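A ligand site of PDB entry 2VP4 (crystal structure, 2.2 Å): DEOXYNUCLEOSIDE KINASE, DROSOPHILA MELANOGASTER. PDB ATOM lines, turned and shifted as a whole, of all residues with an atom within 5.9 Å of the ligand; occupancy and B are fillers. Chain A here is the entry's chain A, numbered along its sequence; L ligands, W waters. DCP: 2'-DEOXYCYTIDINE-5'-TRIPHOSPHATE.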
ATOM      1  N   GLY A  27       0.678 -16.155   0.657  1.00  0.00           N
ATOM      2  CA  GLY A  27       0.506 -17.574   0.360  1.00  0.00           C
ATOM      3  C   GLY A  27       0.680 -17.715  -1.120  1.00  0.00           C
ATOM      4  O   GLY A  27       0.565 -16.740  -1.834  1.00  0.00           O
ATOM      5  N   ASN A  28       0.928 -18.939  -1.582  1.00  0.00           N
ATOM      6  CA  ASN A  28       1.093 -19.238  -3.009  1.00  0.00           C
ATOM      7  C   ASN A  28      -0.115 -18.826  -3.845  1.00  0.00           C
ATOM      8  O   ASN A  28      -1.177 -18.516  -3.284  1.00  0.00           O
ATOM      9  CB  ASN A  28       1.361 -20.737  -3.172  1.00  0.00           C
ATOM     10  CG  ASN A  28       2.243 -21.072  -4.345  1.00  0.00           C
ATOM     11  OD1 ASN A  28       2.442 -20.257  -5.269  1.00  0.00           O
ATOM     12  ND2 ASN A  28       2.763 -22.306  -4.341  1.00  0.00           N
ATOM     13  N   ILE A  29       0.045 -18.827  -5.166  1.00  0.00           N
ATOM     14  CA  ILE A  29      -1.079 -18.621  -6.074  1.00  0.00           C
ATOM     15  C   ILE A  29      -2.108 -19.706  -5.793  1.00  0.00           C
ATOM     16  O   ILE A  29      -1.758 -20.897  -5.703  1.00  0.00           O
ATOM     17  CB  ILE A  29      -0.687 -18.774  -7.584  1.00  0.00           C
ATOM     18  CG1 ILE A  29       0.655 -18.101  -7.913  1.00  0.00           C
ATOM     19  CG2 ILE A  29      -1.825 -18.289  -8.447  1.00  0.00           C
ATOM     20  CD1 ILE A  29       1.140 -18.306  -9.356  1.00  0.00           C
ATOM     21  N   GLY A  30      -3.368 -19.313  -5.677  1.00  0.00           N
ATOM     22  CA  GLY A  30      -4.453 -20.273  -5.458  1.00  0.00           C
ATOM     23  C   GLY A  30      -4.600 -20.741  -4.023  1.00  0.00           C
ATOM     24  O   GLY A  30      -5.321 -21.680  -3.767  1.00  0.00           O
ATOM     25  N   SER A  31      -3.921 -20.080  -3.076  1.00  0.00           N
ATOM     26  CA  SER A  31      -3.902 -20.545  -1.697  1.00  0.00           C
ATOM     27  C   SER A  31      -5.157 -20.134  -0.888  1.00  0.00           C
ATOM     28  O   SER A  31      -5.365 -20.620   0.217  1.00  0.00           O
ATOM     29  CB  SER A  31      -2.587 -20.131  -0.978  1.00  0.00           C
ATOM     30  OG  SER A  31      -2.444 -18.716  -0.802  1.00  0.00           O
ATOM     31  N   GLY A  32      -5.982 -19.260  -1.468  1.00  0.00           N
ATOM     32  CA  GLY A  32      -7.212 -18.808  -0.850  1.00  0.00           C
ATOM     33  C   GLY A  32      -7.086 -17.518  -0.068  1.00  0.00           C
ATOM     34  O   GLY A  32      -7.759 -17.343   0.944  1.00  0.00           O
ATOM     35  N   LYS A  33      -6.254 -16.586  -0.559  1.00  0.00           N
ATOM     36  CA  LYS A  33      -6.031 -15.303   0.129  1.00  0.00           C
ATOM     37  C   LYS A  33      -7.239 -14.369   0.116  1.00  0.00           C
ATOM     38  O   LYS A  33      -7.559 -13.730   1.116  1.00  0.00           O
ATOM     39  CB  LYS A  33      -4.787 -14.591  -0.427  1.00  0.00           C
ATOM     40  CG  LYS A  33      -3.479 -15.325  -0.198  1.00  0.00           C
ATOM     41  CD  LYS A  33      -2.288 -14.602  -0.851  1.00  0.00           C
ATOM     42  CE  LYS A  33      -2.398 -14.513  -2.366  1.00  0.00           C
ATOM     43  NZ  LYS A  33      -2.297 -15.855  -3.018  1.00  0.00           N
ATOM     44  N   THR A  34      -7.897 -14.266  -1.024  1.00  0.00           N
ATOM     45  CA  THR A  34      -9.088 -13.424  -1.155  1.00  0.00           C
ATOM     46  C   THR A  34     -10.268 -14.041  -0.355  1.00  0.00           C
ATOM     47  O   THR A  34     -10.976 -13.329   0.353  1.00  0.00           O
ATOM     48  CB  THR A  34      -9.457 -13.241  -2.628  1.00  0.00           C
ATOM     49  OG1 THR A  34      -8.303 -12.812  -3.357  1.00  0.00           O
ATOM     50  CG2 THR A  34     -10.566 -12.206  -2.791  1.00  0.00           C
ATOM     51  N   THR A  35     -10.444 -15.361  -0.465  1.00  0.00           N
ATOM     52  CA  THR A  35     -11.448 -16.083   0.327  1.00  0.00           C
ATOM     53  C   THR A  35     -11.306 -15.826   1.825  1.00  0.00           C
ATOM     54  O   THR A  35     -12.264 -15.432   2.497  1.00  0.00           O
ATOM     55  CB  THR A  35     -11.365 -17.602   0.062  1.00  0.00           C
ATOM     56  OG1 THR A  35     -11.465 -17.837  -1.338  1.00  0.00           O
ATOM     57  CG2 THR A  35     -12.492 -18.356   0.789  1.00  0.00           C
ATOM     58  N   GLU A  52      -8.382  -7.800  -4.082  1.00  0.00           N
ATOM     59  CA  GLU A  52      -7.418  -8.785  -4.456  1.00  0.00           C
ATOM     60  C   GLU A  52      -6.752  -7.946  -5.574  1.00  0.00           C
ATOM     61  O   GLU A  52      -7.406  -7.557  -6.551  1.00  0.00           O
ATOM     62  CB  GLU A  52      -8.158  -9.962  -5.088  1.00  0.00           C
ATOM     63  CG  GLU A  52      -9.397  -9.532  -5.879  1.00  0.00           C
ATOM     64  CD  GLU A  52     -10.259 -10.683  -6.385  1.00  0.00           C
ATOM     65  OE1 GLU A  52     -11.491 -10.551  -6.205  1.00  0.00           O
ATOM     66  OE2 GLU A  52      -9.742 -11.697  -6.954  1.00  0.00           O
ATOM     67  N   PRO A  53      -5.457  -7.616  -5.412  1.00  0.00           N
ATOM     68  CA  PRO A  53      -4.825  -6.658  -6.335  1.00  0.00           C
ATOM     69  C   PRO A  53      -4.752  -7.119  -7.798  1.00  0.00           C
ATOM     70  O   PRO A  53      -4.580  -6.286  -8.653  1.00  0.00           O
ATOM     71  CB  PRO A  53      -3.411  -6.496  -5.753  1.00  0.00           C
ATOM     72  CG  PRO A  53      -3.190  -7.781  -4.959  1.00  0.00           C
ATOM     73  CD  PRO A  53      -4.540  -8.074  -4.362  1.00  0.00           C
ATOM     74  N   VAL A  54      -4.891  -8.425  -8.069  1.00  0.00           N
ATOM     75  CA  VAL A  54      -4.793  -8.950  -9.440  1.00  0.00           C
ATOM     76  C   VAL A  54      -5.794  -8.299 -10.396  1.00  0.00           C
ATOM     77  O   VAL A  54      -5.547  -8.167 -11.603  1.00  0.00           O
ATOM     78  CB  VAL A  54      -4.871 -10.501  -9.498  1.00  0.00           C
ATOM     79  CG1 VAL A  54      -6.282 -11.022  -9.130  1.00  0.00           C
ATOM     80  CG2 VAL A  54      -4.439 -11.007 -10.847  1.00  0.00           C
ATOM     81  N   TRP A  57      -4.028  -5.615 -12.077  1.00  0.00           N
ATOM     82  CA  TRP A  57      -2.962  -6.016 -13.008  1.00  0.00           C
ATOM     83  C   TRP A  57      -3.524  -6.511 -14.349  1.00  0.00           C
ATOM     84  O   TRP A  57      -2.852  -6.465 -15.384  1.00  0.00           O
ATOM     85  CB  TRP A  57      -2.022  -7.037 -12.369  1.00  0.00           C
ATOM     86  CG  TRP A  57      -1.596  -6.694 -10.956  1.00  0.00           C
ATOM     87  CD1 TRP A  57      -1.482  -5.446 -10.412  1.00  0.00           C
ATOM     88  CD2 TRP A  57      -1.250  -7.620  -9.915  1.00  0.00           C
ATOM     89  NE1 TRP A  57      -1.093  -5.537  -9.093  1.00  0.00           N
ATOM     90  CE2 TRP A  57      -0.928  -6.855  -8.762  1.00  0.00           C
ATOM     91  CE3 TRP A  57      -1.170  -9.015  -9.842  1.00  0.00           C
ATOM     92  CZ2 TRP A  57      -0.540  -7.446  -7.550  1.00  0.00           C
ATOM     93  CZ3 TRP A  57      -0.773  -9.610  -8.626  1.00  0.00           C
ATOM     94  CH2 TRP A  57      -0.468  -8.825  -7.500  1.00  0.00           C
ATOM     95  N   LEU A  66      -0.902  -8.861 -16.750  1.00  0.00           N
ATOM     96  CA  LEU A  66      -0.760 -10.242 -16.285  1.00  0.00           C
ATOM     97  C   LEU A  66      -0.745 -11.203 -17.491  1.00  0.00           C
ATOM     98  O   LEU A  66       0.055 -12.129 -17.550  1.00  0.00           O
ATOM     99  CB  LEU A  66      -1.933 -10.613 -15.344  1.00  0.00           C
ATOM    100  CG  LEU A  66      -1.890 -12.028 -14.724  1.00  0.00           C
ATOM    101  CD1 LEU A  66      -0.743 -12.203 -13.653  1.00  0.00           C
ATOM    102  CD2 LEU A  66      -3.240 -12.406 -14.120  1.00  0.00           C
ATOM    103  N   MET A  69       2.494 -10.712 -19.512  1.00  0.00           N
ATOM    104  CA  MET A  69       3.617 -11.292 -18.803  1.00  0.00           C
ATOM    105  C   MET A  69       3.700 -12.789 -19.011  1.00  0.00           C
ATOM    106  O   MET A  69       4.776 -13.315 -19.287  1.00  0.00           O
ATOM    107  CB  MET A  69       3.537 -10.932 -17.299  1.00  0.00           C
ATOM    108  CG  MET A  69       4.649 -11.536 -16.422  1.00  0.00           C
ATOM    109  SD  MET A  69       4.267 -13.205 -15.874  1.00  0.00           S
ATOM    110  CE  MET A  69       2.955 -12.903 -14.689  1.00  0.00           C
ATOM    111  N   TYR A  70       2.590 -13.491 -18.901  1.00  0.00           N
ATOM    112  CA  TYR A  70       2.591 -14.948 -19.119  1.00  0.00           C
ATOM    113  C   TYR A  70       2.878 -15.321 -20.557  1.00  0.00           C
ATOM    114  O   TYR A  70       3.578 -16.307 -20.814  1.00  0.00           O
ATOM    115  CB  TYR A  70       1.269 -15.595 -18.660  1.00  0.00           C
ATOM    116  CG  TYR A  70       1.258 -15.802 -17.177  1.00  0.00           C
ATOM    117  CD1 TYR A  70       0.249 -15.279 -16.378  1.00  0.00           C
ATOM    118  CD2 TYR A  70       2.269 -16.531 -16.564  1.00  0.00           C
ATOM    119  CE1 TYR A  70       0.248 -15.502 -14.979  1.00  0.00           C
ATOM    120  CE2 TYR A  70       2.284 -16.742 -15.195  1.00  0.00           C
ATOM    121  CZ  TYR A  70       1.277 -16.229 -14.413  1.00  0.00           C
ATOM    122  OH  TYR A  70       1.315 -16.469 -13.047  1.00  0.00           O
ATOM    123  N   PHE A  80       5.474  -5.659 -15.723  1.00  0.00           N
ATOM    124  CA  PHE A  80       4.469  -6.271 -14.811  1.00  0.00           C
ATOM    125  C   PHE A  80       4.810  -6.156 -13.296  1.00  0.00           C
ATOM    126  O   PHE A  80       4.031  -5.647 -12.499  1.00  0.00           O
ATOM    127  CB  PHE A  80       4.199  -7.737 -15.195  1.00  0.00           C
ATOM    128  CG  PHE A  80       3.229  -8.411 -14.288  1.00  0.00           C
ATOM    129  CD1 PHE A  80       1.879  -8.148 -14.373  1.00  0.00           C
ATOM    130  CD2 PHE A  80       3.677  -9.287 -13.328  1.00  0.00           C
ATOM    131  CE1 PHE A  80       0.976  -8.762 -13.497  1.00  0.00           C
ATOM    132  CE2 PHE A  80       2.762  -9.911 -12.459  1.00  0.00           C
ATOM    133  CZ  PHE A  80       1.423  -9.620 -12.549  1.00  0.00           C
ATOM    134  N   GLN A  81       5.990  -6.635 -12.910  1.00  0.00           N
ATOM    135  CA  GLN A  81       6.419  -6.571 -11.508  1.00  0.00           C
ATOM    136  C   GLN A  81       6.585  -5.125 -11.038  1.00  0.00           C
ATOM    137  O   GLN A  81       6.404  -4.796  -9.860  1.00  0.00           O
ATOM    138  CB  GLN A  81       7.722  -7.342 -11.303  1.00  0.00           C
ATOM    139  CG  GLN A  81       7.635  -8.849 -11.449  1.00  0.00           C
ATOM    140  CD  GLN A  81       6.571  -9.517 -10.556  1.00  0.00           C
ATOM    141  OE1 GLN A  81       6.064 -10.571 -10.884  1.00  0.00           O
ATOM    142  NE2 GLN A  81       6.244  -8.905  -9.432  1.00  0.00           N
ATOM    143  N   VAL A  84       3.058  -4.104 -10.192  1.00  0.00           N
ATOM    144  CA  VAL A  84       2.671  -4.819  -8.970  1.00  0.00           C
ATOM    145  C   VAL A  84       3.233  -4.062  -7.775  1.00  0.00           C
ATOM    146  O   VAL A  84       2.497  -3.666  -6.865  1.00  0.00           O
ATOM    147  CB  VAL A  84       3.157  -6.314  -8.981  1.00  0.00           C
ATOM    148  CG1 VAL A  84       2.999  -6.971  -7.616  1.00  0.00           C
ATOM    149  CG2 VAL A  84       2.443  -7.120 -10.077  1.00  0.00           C
ATOM    150  N   GLU A 104      -4.241  -8.034   0.963  1.00  0.00           N
ATOM    151  CA  GLU A 104      -3.812  -9.197   0.230  1.00  0.00           C
ATOM    152  C   GLU A 104      -2.464  -8.891  -0.412  1.00  0.00           C
ATOM    153  O   GLU A 104      -2.322  -7.909  -1.152  1.00  0.00           O
ATOM    154  CB  GLU A 104      -4.801  -9.608  -0.852  1.00  0.00           C
ATOM    155  CG  GLU A 104      -4.431 -10.979  -1.469  1.00  0.00           C
ATOM    156  CD  GLU A 104      -5.547 -11.526  -2.356  1.00  0.00           C
ATOM    157  OE1 GLU A 104      -6.697 -11.078  -2.241  1.00  0.00           O
ATOM    158  OE2 GLU A 104      -5.257 -12.415  -3.174  1.00  0.00           O
ATOM    159  N   ARG A 105      -1.500  -9.742  -0.119  1.00  0.00           N
ATOM    160  CA  ARG A 105      -0.141  -9.611  -0.587  1.00  0.00           C
ATOM    161  C   ARG A 105       0.548  -8.342  -0.068  1.00  0.00           C
ATOM    162  O   ARG A 105       0.038  -7.653   0.856  1.00  0.00           O
ATOM    163  CB  ARG A 105      -0.037  -9.785  -2.125  1.00  0.00           C
ATOM    164  CG  ARG A 105      -0.316 -11.231  -2.594  1.00  0.00           C
ATOM    165  CD  ARG A 105       0.765 -11.695  -3.507  1.00  0.00           C
ATOM    166  NE  ARG A 105       0.567 -13.032  -4.063  1.00  0.00           N
ATOM    167  CZ  ARG A 105       1.199 -14.121  -3.640  1.00  0.00           C
ATOM    168  NH1 ARG A 105       2.043 -14.054  -2.602  1.00  0.00           N
ATOM    169  NH2 ARG A 105       0.971 -15.289  -4.223  1.00  0.00           N
ATOM    170  N   SER A 109       6.415 -10.043  -1.160  1.00  0.00           N
ATOM    171  CA  SER A 109       6.322 -11.279  -1.949  1.00  0.00           C
ATOM    172  C   SER A 109       6.702 -11.037  -3.392  1.00  0.00           C
ATOM    173  O   SER A 109       7.278 -11.913  -4.021  1.00  0.00           O
ATOM    174  CB  SER A 109       4.957 -11.980  -1.843  1.00  0.00           C
ATOM    175  OG  SER A 109       3.846 -11.095  -1.934  1.00  0.00           O
ATOM    176  N   ALA A 110       6.377  -9.848  -3.920  1.00  0.00           N
ATOM    177  CA  ALA A 110       6.840  -9.462  -5.256  1.00  0.00           C
ATOM    178  C   ALA A 110       8.375  -9.589  -5.335  1.00  0.00           C
ATOM    179  O   ALA A 110       8.927 -10.292  -6.198  1.00  0.00           O
ATOM    180  CB  ALA A 110       6.372  -8.025  -5.589  1.00  0.00           C
ATOM    181  N   PHE A 114       8.269 -13.553  -6.322  1.00  0.00           N
ATOM    182  CA  PHE A 114       8.003 -13.489  -7.767  1.00  0.00           C
ATOM    183  C   PHE A 114       9.143 -12.931  -8.641  1.00  0.00           C
ATOM    184  O   PHE A 114       9.520 -13.557  -9.631  1.00  0.00           O
ATOM    185  CB  PHE A 114       6.661 -12.820  -8.030  1.00  0.00           C
ATOM    186  CG  PHE A 114       5.485 -13.656  -7.577  1.00  0.00           C
ATOM    187  CD1 PHE A 114       5.022 -13.584  -6.274  1.00  0.00           C
ATOM    188  CD2 PHE A 114       4.856 -14.512  -8.453  1.00  0.00           C
ATOM    189  CE1 PHE A 114       3.943 -14.344  -5.860  1.00  0.00           C
ATOM    190  CE2 PHE A 114       3.788 -15.261  -8.057  1.00  0.00           C
ATOM    191  CZ  PHE A 114       3.325 -15.189  -6.754  1.00  0.00           C
ATOM    192  N   VAL A 115       9.722 -11.802  -8.246  1.00  0.00           N
ATOM    193  CA  VAL A 115      10.888 -11.229  -8.984  1.00  0.00           C
ATOM    194  C   VAL A 115      12.087 -12.211  -8.929  1.00  0.00           C
ATOM    195  O   VAL A 115      12.694 -12.504  -9.942  1.00  0.00           O
ATOM    196  CB  VAL A 115      11.279  -9.817  -8.421  1.00  0.00           C
ATOM    197  CG1 VAL A 115      12.675  -9.306  -8.951  1.00  0.00           C
ATOM    198  CG2 VAL A 115      10.203  -8.814  -8.716  1.00  0.00           C
ATOM    199  N   MET A 118      11.481 -15.192 -11.296  1.00  0.00           N
ATOM    200  CA  MET A 118      11.614 -14.761 -12.697  1.00  0.00           C
ATOM    201  C   MET A 118      13.077 -14.527 -13.065  1.00  0.00           C
ATOM    202  O   MET A 118      13.481 -14.828 -14.178  1.00  0.00           O
ATOM    203  CB  MET A 118      10.729 -13.567 -12.988  1.00  0.00           C
ATOM    204  CG  MET A 118       9.253 -13.941 -12.961  1.00  0.00           C
ATOM    205  SD  MET A 118       8.197 -12.573 -13.383  1.00  0.00           S
ATOM    206  CE  MET A 118       6.565 -13.240 -12.884  1.00  0.00           C
ATOM    207  N   LEU A 153      -0.942 -18.343   4.470  1.00  0.00           N
ATOM    208  CA  LEU A 153      -1.810 -19.461   4.145  1.00  0.00           C
ATOM    209  C   LEU A 153      -0.987 -20.527   3.474  1.00  0.00           C
ATOM    210  O   LEU A 153      -0.809 -20.503   2.258  1.00  0.00           O
ATOM    211  CB  LEU A 153      -3.000 -19.018   3.291  1.00  0.00           C
ATOM    212  CG  LEU A 153      -3.810 -17.811   3.777  1.00  0.00           C
ATOM    213  CD1 LEU A 153      -4.966 -17.542   2.836  1.00  0.00           C
ATOM    214  CD2 LEU A 153      -4.357 -17.951   5.232  1.00  0.00           C
ATOM    215  N   ARG A 167     -10.187 -22.717 -10.995  1.00  0.00           N
ATOM    216  CA  ARG A 167     -10.511 -21.306 -11.188  1.00  0.00           C
ATOM    217  C   ARG A 167     -10.492 -20.968 -12.683  1.00  0.00           C
ATOM    218  O   ARG A 167     -11.373 -20.251 -13.168  1.00  0.00           O
ATOM    219  CB  ARG A 167      -9.500 -20.454 -10.389  1.00  0.00           C
ATOM    220  CG  ARG A 167      -9.751 -18.957 -10.344  1.00  0.00           C
ATOM    221  CD  ARG A 167      -8.827 -18.279  -9.310  1.00  0.00           C
ATOM    222  NE  ARG A 167      -7.385 -18.389  -9.625  1.00  0.00           N
ATOM    223  CZ  ARG A 167      -6.412 -18.181  -8.749  1.00  0.00           C
ATOM    224  NH1 ARG A 167      -6.679 -17.859  -7.491  1.00  0.00           N
ATOM    225  NH2 ARG A 167      -5.150 -18.269  -9.133  1.00  0.00           N
ATOM    226  N   ARG A 169      -8.541 -18.995 -14.650  1.00  0.00           N
ATOM    227  CA  ARG A 169      -8.196 -17.720 -15.246  1.00  0.00           C
ATOM    228  C   ARG A 169      -7.447 -18.033 -16.531  1.00  0.00           C
ATOM    229  O   ARG A 169      -6.495 -18.808 -16.516  1.00  0.00           O
ATOM    230  CB  ARG A 169      -7.274 -16.908 -14.359  1.00  0.00           C
ATOM    231  CG  ARG A 169      -7.836 -16.517 -13.046  1.00  0.00           C
ATOM    232  CD  ARG A 169      -7.061 -15.298 -12.508  1.00  0.00           C
ATOM    233  NE  ARG A 169      -7.592 -14.957 -11.207  1.00  0.00           N
ATOM    234  CZ  ARG A 169      -6.923 -15.007 -10.077  1.00  0.00           C
ATOM    235  NH1 ARG A 169      -5.635 -15.335 -10.076  1.00  0.00           N
ATOM    236  NH2 ARG A 169      -7.531 -14.695  -8.944  1.00  0.00           N
ATOM    237  N   GLU A 172      -3.590 -17.759 -16.697  1.00  0.00           N
ATOM    238  CA  GLU A 172      -2.811 -18.753 -15.949  1.00  0.00           C
ATOM    239  C   GLU A 172      -2.844 -20.173 -16.553  1.00  0.00           C
ATOM    240  O   GLU A 172      -2.373 -21.136 -15.917  1.00  0.00           O
ATOM    241  CB  GLU A 172      -3.274 -18.786 -14.494  1.00  0.00           C
ATOM    242  CG  GLU A 172      -3.178 -17.429 -13.783  1.00  0.00           C
ATOM    243  CD  GLU A 172      -3.830 -17.423 -12.422  1.00  0.00           C
ATOM    244  OE1 GLU A 172      -4.547 -18.388 -12.076  1.00  0.00           O
ATOM    245  OE2 GLU A 172      -3.626 -16.427 -11.693  1.00  0.00           O
ATOM    246  N   VAL A 175       0.460 -22.261 -16.708  1.00  0.00           N
ATOM    247  CA  VAL A 175       1.266 -22.294 -15.503  1.00  0.00           C
ATOM    248  C   VAL A 175       1.410 -23.758 -15.067  1.00  0.00           C
ATOM    249  O   VAL A 175       0.411 -24.451 -14.880  1.00  0.00           O
ATOM    250  CB  VAL A 175       0.636 -21.405 -14.375  1.00  0.00           C
ATOM    251  CG1 VAL A 175       1.378 -21.562 -13.048  1.00  0.00           C
ATOM    252  CG2 VAL A 175       0.624 -19.922 -14.784  1.00  0.00           C
ATOM    253  N   TYR A 179       6.284 -24.470 -11.406  1.00  0.00           N
ATOM    254  CA  TYR A 179       6.304 -23.054 -11.063  1.00  0.00           C
ATOM    255  C   TYR A 179       5.744 -22.799  -9.673  1.00  0.00           C
ATOM    256  O   TYR A 179       6.267 -21.966  -8.937  1.00  0.00           O
ATOM    257  CB  TYR A 179       5.500 -22.280 -12.102  1.00  0.00           C
ATOM    258  CG  TYR A 179       5.600 -20.765 -12.019  1.00  0.00           C
ATOM    259  CD1 TYR A 179       6.814 -20.103 -12.247  1.00  0.00           C
ATOM    260  CD2 TYR A 179       4.466 -19.984 -11.758  1.00  0.00           C
ATOM    261  CE1 TYR A 179       6.893 -18.721 -12.212  1.00  0.00           C
ATOM    262  CE2 TYR A 179       4.548 -18.583 -11.711  1.00  0.00           C
ATOM    263  CZ  TYR A 179       5.761 -17.964 -11.948  1.00  0.00           C
ATOM    264  OH  TYR A 179       5.843 -16.587 -11.896  1.00  0.00           O
HETATM  265  N1  DCP L   1       1.630 -12.697  -9.570  1.00  0.00           N
HETATM  266  C2  DCP L   1       2.894 -12.362 -10.132  1.00  0.00           C
HETATM  267  N3  DCP L   1       3.704 -11.529  -9.450  1.00  0.00           N
HETATM  268  C4  DCP L   1       3.367 -11.021  -8.248  1.00  0.00           C
HETATM  269  C5  DCP L   1       2.128 -11.336  -7.672  1.00  0.00           C
HETATM  270  C6  DCP L   1       1.271 -12.171  -8.382  1.00  0.00           C
HETATM  271  O2  DCP L   1       3.267 -12.838 -11.243  1.00  0.00           O
HETATM  272  N4  DCP L   1       4.231 -10.210  -7.617  1.00  0.00           N
HETATM  273  C1' DCP L   1       0.704 -13.522 -10.330  1.00  0.00           C
HETATM  274  C2' DCP L   1       0.409 -14.960  -9.921  1.00  0.00           C
HETATM  275  C3' DCP L   1      -1.045 -15.103 -10.401  1.00  0.00           C
HETATM  276  C4' DCP L   1      -1.657 -13.724 -10.245  1.00  0.00           C
HETATM  277  O4' DCP L   1      -0.553 -12.827 -10.290  1.00  0.00           O
HETATM  278  O3' DCP L   1      -1.069 -15.411 -11.806  1.00  0.00           O
HETATM  279  C5' DCP L   1      -2.324 -13.521  -8.892  1.00  0.00           C
HETATM  280  O5' DCP L   1      -1.702 -14.376  -7.927  1.00  0.00           O
HETATM  281  PA  DCP L   1      -1.915 -14.099  -6.384  1.00  0.00           P
HETATM  282  O1A DCP L   1      -1.420 -12.701  -6.075  1.00  0.00           O
HETATM  283  O2A DCP L   1      -1.336 -15.217  -5.576  1.00  0.00           O
HETATM  284  O3A DCP L   1      -3.510 -13.943  -6.293  1.00  0.00           O
HETATM  285  PB  DCP L   1      -4.644 -15.090  -6.329  1.00  0.00           P
HETATM  286  O1B DCP L   1      -4.198 -16.198  -7.215  1.00  0.00           O
HETATM  287  O2B DCP L   1      -5.905 -14.332  -6.605  1.00  0.00           O
HETATM  288  O3B DCP L   1      -4.625 -15.540  -4.769  1.00  0.00           O
HETATM  289  PG  DCP L   1      -5.712 -16.495  -4.015  1.00  0.00           P
HETATM  290  O1G DCP L   1      -6.749 -15.531  -3.612  1.00  0.00           O
HETATM  291  O2G DCP L   1      -4.856 -17.067  -2.910  1.00  0.00           O
HETATM  292  O3G DCP L   1      -6.124 -17.509  -5.041  1.00  0.00           O
HETATM  293  O   HOH W   1      -7.936 -19.480  -4.101  1.00  0.00           O
HETATM  294  O   HOH W   2      -8.943 -17.032  -2.657  1.00  0.00           O
HETATM  295  O   HOH W   3       3.244  -9.395  -4.542  1.00  0.00           O
HETATM  296  O   HOH W   4       3.604 -15.621 -11.836  1.00  0.00           O
HETATM  297  O   HOH W   5      -3.133 -11.334  -4.605  1.00  0.00           O
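An oxygen (O2A) of the ligand is in salt-bridge range of the side-chain amino group (NZ) of Lys 33 (2.8 Å).
An oxygen (O3') of the ligand sits at hydrogen-bond distance from the side-chain carboxylate (OE2) of Glu 172, at 2.8 Å.
An oxygen (O2G) of the ligand is in hydrogen-bond range of the backbone NH (N) of Gly 32.
An oxygen (O2B) of the ligand is in salt-bridge range of the guanidinium group (NH2) of Arg 169, at 2.9 Å.
The backbone NH of Gly 30 lies close to an oxygen (O3G) of the ligand, 3.4 Å away.
N of Lys 33 sits at hydrogen-bond distance from O2G of the ligand.
The side-chain hydroxyl (OH) of Tyr 70 sits at hydrogen-bond distance from an oxygen (O3') of the ligand, 2.9 Å away.
N of Ser 31 is in hydrogen-bond range of O2G of the ligand, 3.2 Å away.
OG1 of Thr 34 lies within hydrogen-bond range of O1G of the ligand, 3.1 Å away.
O1G of the ligand lies within hydrogen-bond range of N of Thr 34 (3.1 Å).
An oxygen (O3G) of the ligand lies within salt-bridge range of the guanidinium group (NH1) of Arg 167 (2.5 Å).
An oxygen (O2A) of the ligand is in salt-bridge range of the guanidinium group (NH2) of Arg 105, at 2.7 Å.
The side-chain amide oxygen (OE1) of Gln 81 lies close to a nitrogen (N3) of the ligand.
NH2 of Arg 105 is in hydrogen-bond range of O of Gly 27 (2.8 Å).
The side-chain hydroxyl (OG) of Ser 31 lies within hydrogen-bond range of the backbone carbonyl oxygen (O) of Asn 28.
The backbone carbonyl oxygen (O) of Trp 57 is in hydrogen-bond range of the backbone NH (N) of Leu 66, at 3.4 Å.
The backbone carbonyl oxygen (O) of Ala 110 is in hydrogen-bond range of the backbone NH (N) of Val 115, at 2.7 Å.
NZ of Lys 33 lies within hydrogen-bond range of O of Asn 28 (2.9 Å).
The side-chain carboxylate (OE2) of Glu 172 lies within salt-bridge range of the guanidinium group (NH1) of Arg 169.
The guanidinium group (NH2) of Arg 167 lies within salt-bridge range of the side-chain carboxylate (OE1) of Glu 172, 3.0 Å away.
O of Ser 109 is in hydrogen-bond range of N of Phe 114, at 3.0 Å.
An oxygen (O1G) of the ligand sits close to the side-chain carboxylate (OE2) of Glu 104 (3.5 Å).
Asn 28 touches the ligand.
Ile 29 touches the ligand.
Val 54 touches the ligand (CG2 to C5', 3.8 Å).
Trp 57 touches the ligand.
Leu 66 touches the ligand.
Met 69 touches the ligand (CE to O2, 3.5 Å).
Phe 80 touches the ligand.
Val 84 touches the ligand.
CA of Ala 110 touches N4 of the ligand, 3.6 Å away.
Phe 114 touches the ligand.
Met 118 touches the ligand (CE to O2, 3.7 Å).
Hydrophobic or aromatic side chains that line the ligand: Ile 29, Val 54, Trp 57, Leu 66, Met 69, Tyr 70, Phe 80, Val 84, Ala 110, Phe 114 and Met 118.
Within 4 Å of the ligand: Asn 28, Ile 29, Gly 30, Ser 31, Gly 32, Lys 33, Thr 34, Val 54, Trp 57, Leu 66, Met 69, Tyr 70, Phe 80, Gln 81, Val 84, Glu 104, Arg 105, Ala 110, Phe 114, Met 118, Arg 167, Arg 169 and Glu 172.
Water W5 lies within hydrogen-bond range of O1A of the ligand and OE2 of Glu 104.
Water W2 lies within hydrogen-bond range of O1G of the ligand (2.8 Å), OG1 of Thr 35 (3.0 Å), N of Thr 34 (3.4 Å) and N of Lys 33 (3.4 Å).
Water W1 lies within hydrogen-bond range of O3G of the ligand (2.8 Å), N of Gly 32 (3.3 Å) and O of Gly 30 (3.4 Å).
Water W4 lies within hydrogen-bond range of OH of Tyr 179 (2.4 Å), OH of Tyr 70 (2.7 Å) and O2 of the ligand (2.9 Å).
Water W3 lies within hydrogen-bond range of OG of Ser 109, N of Ala 110 and N4 of the ligand.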
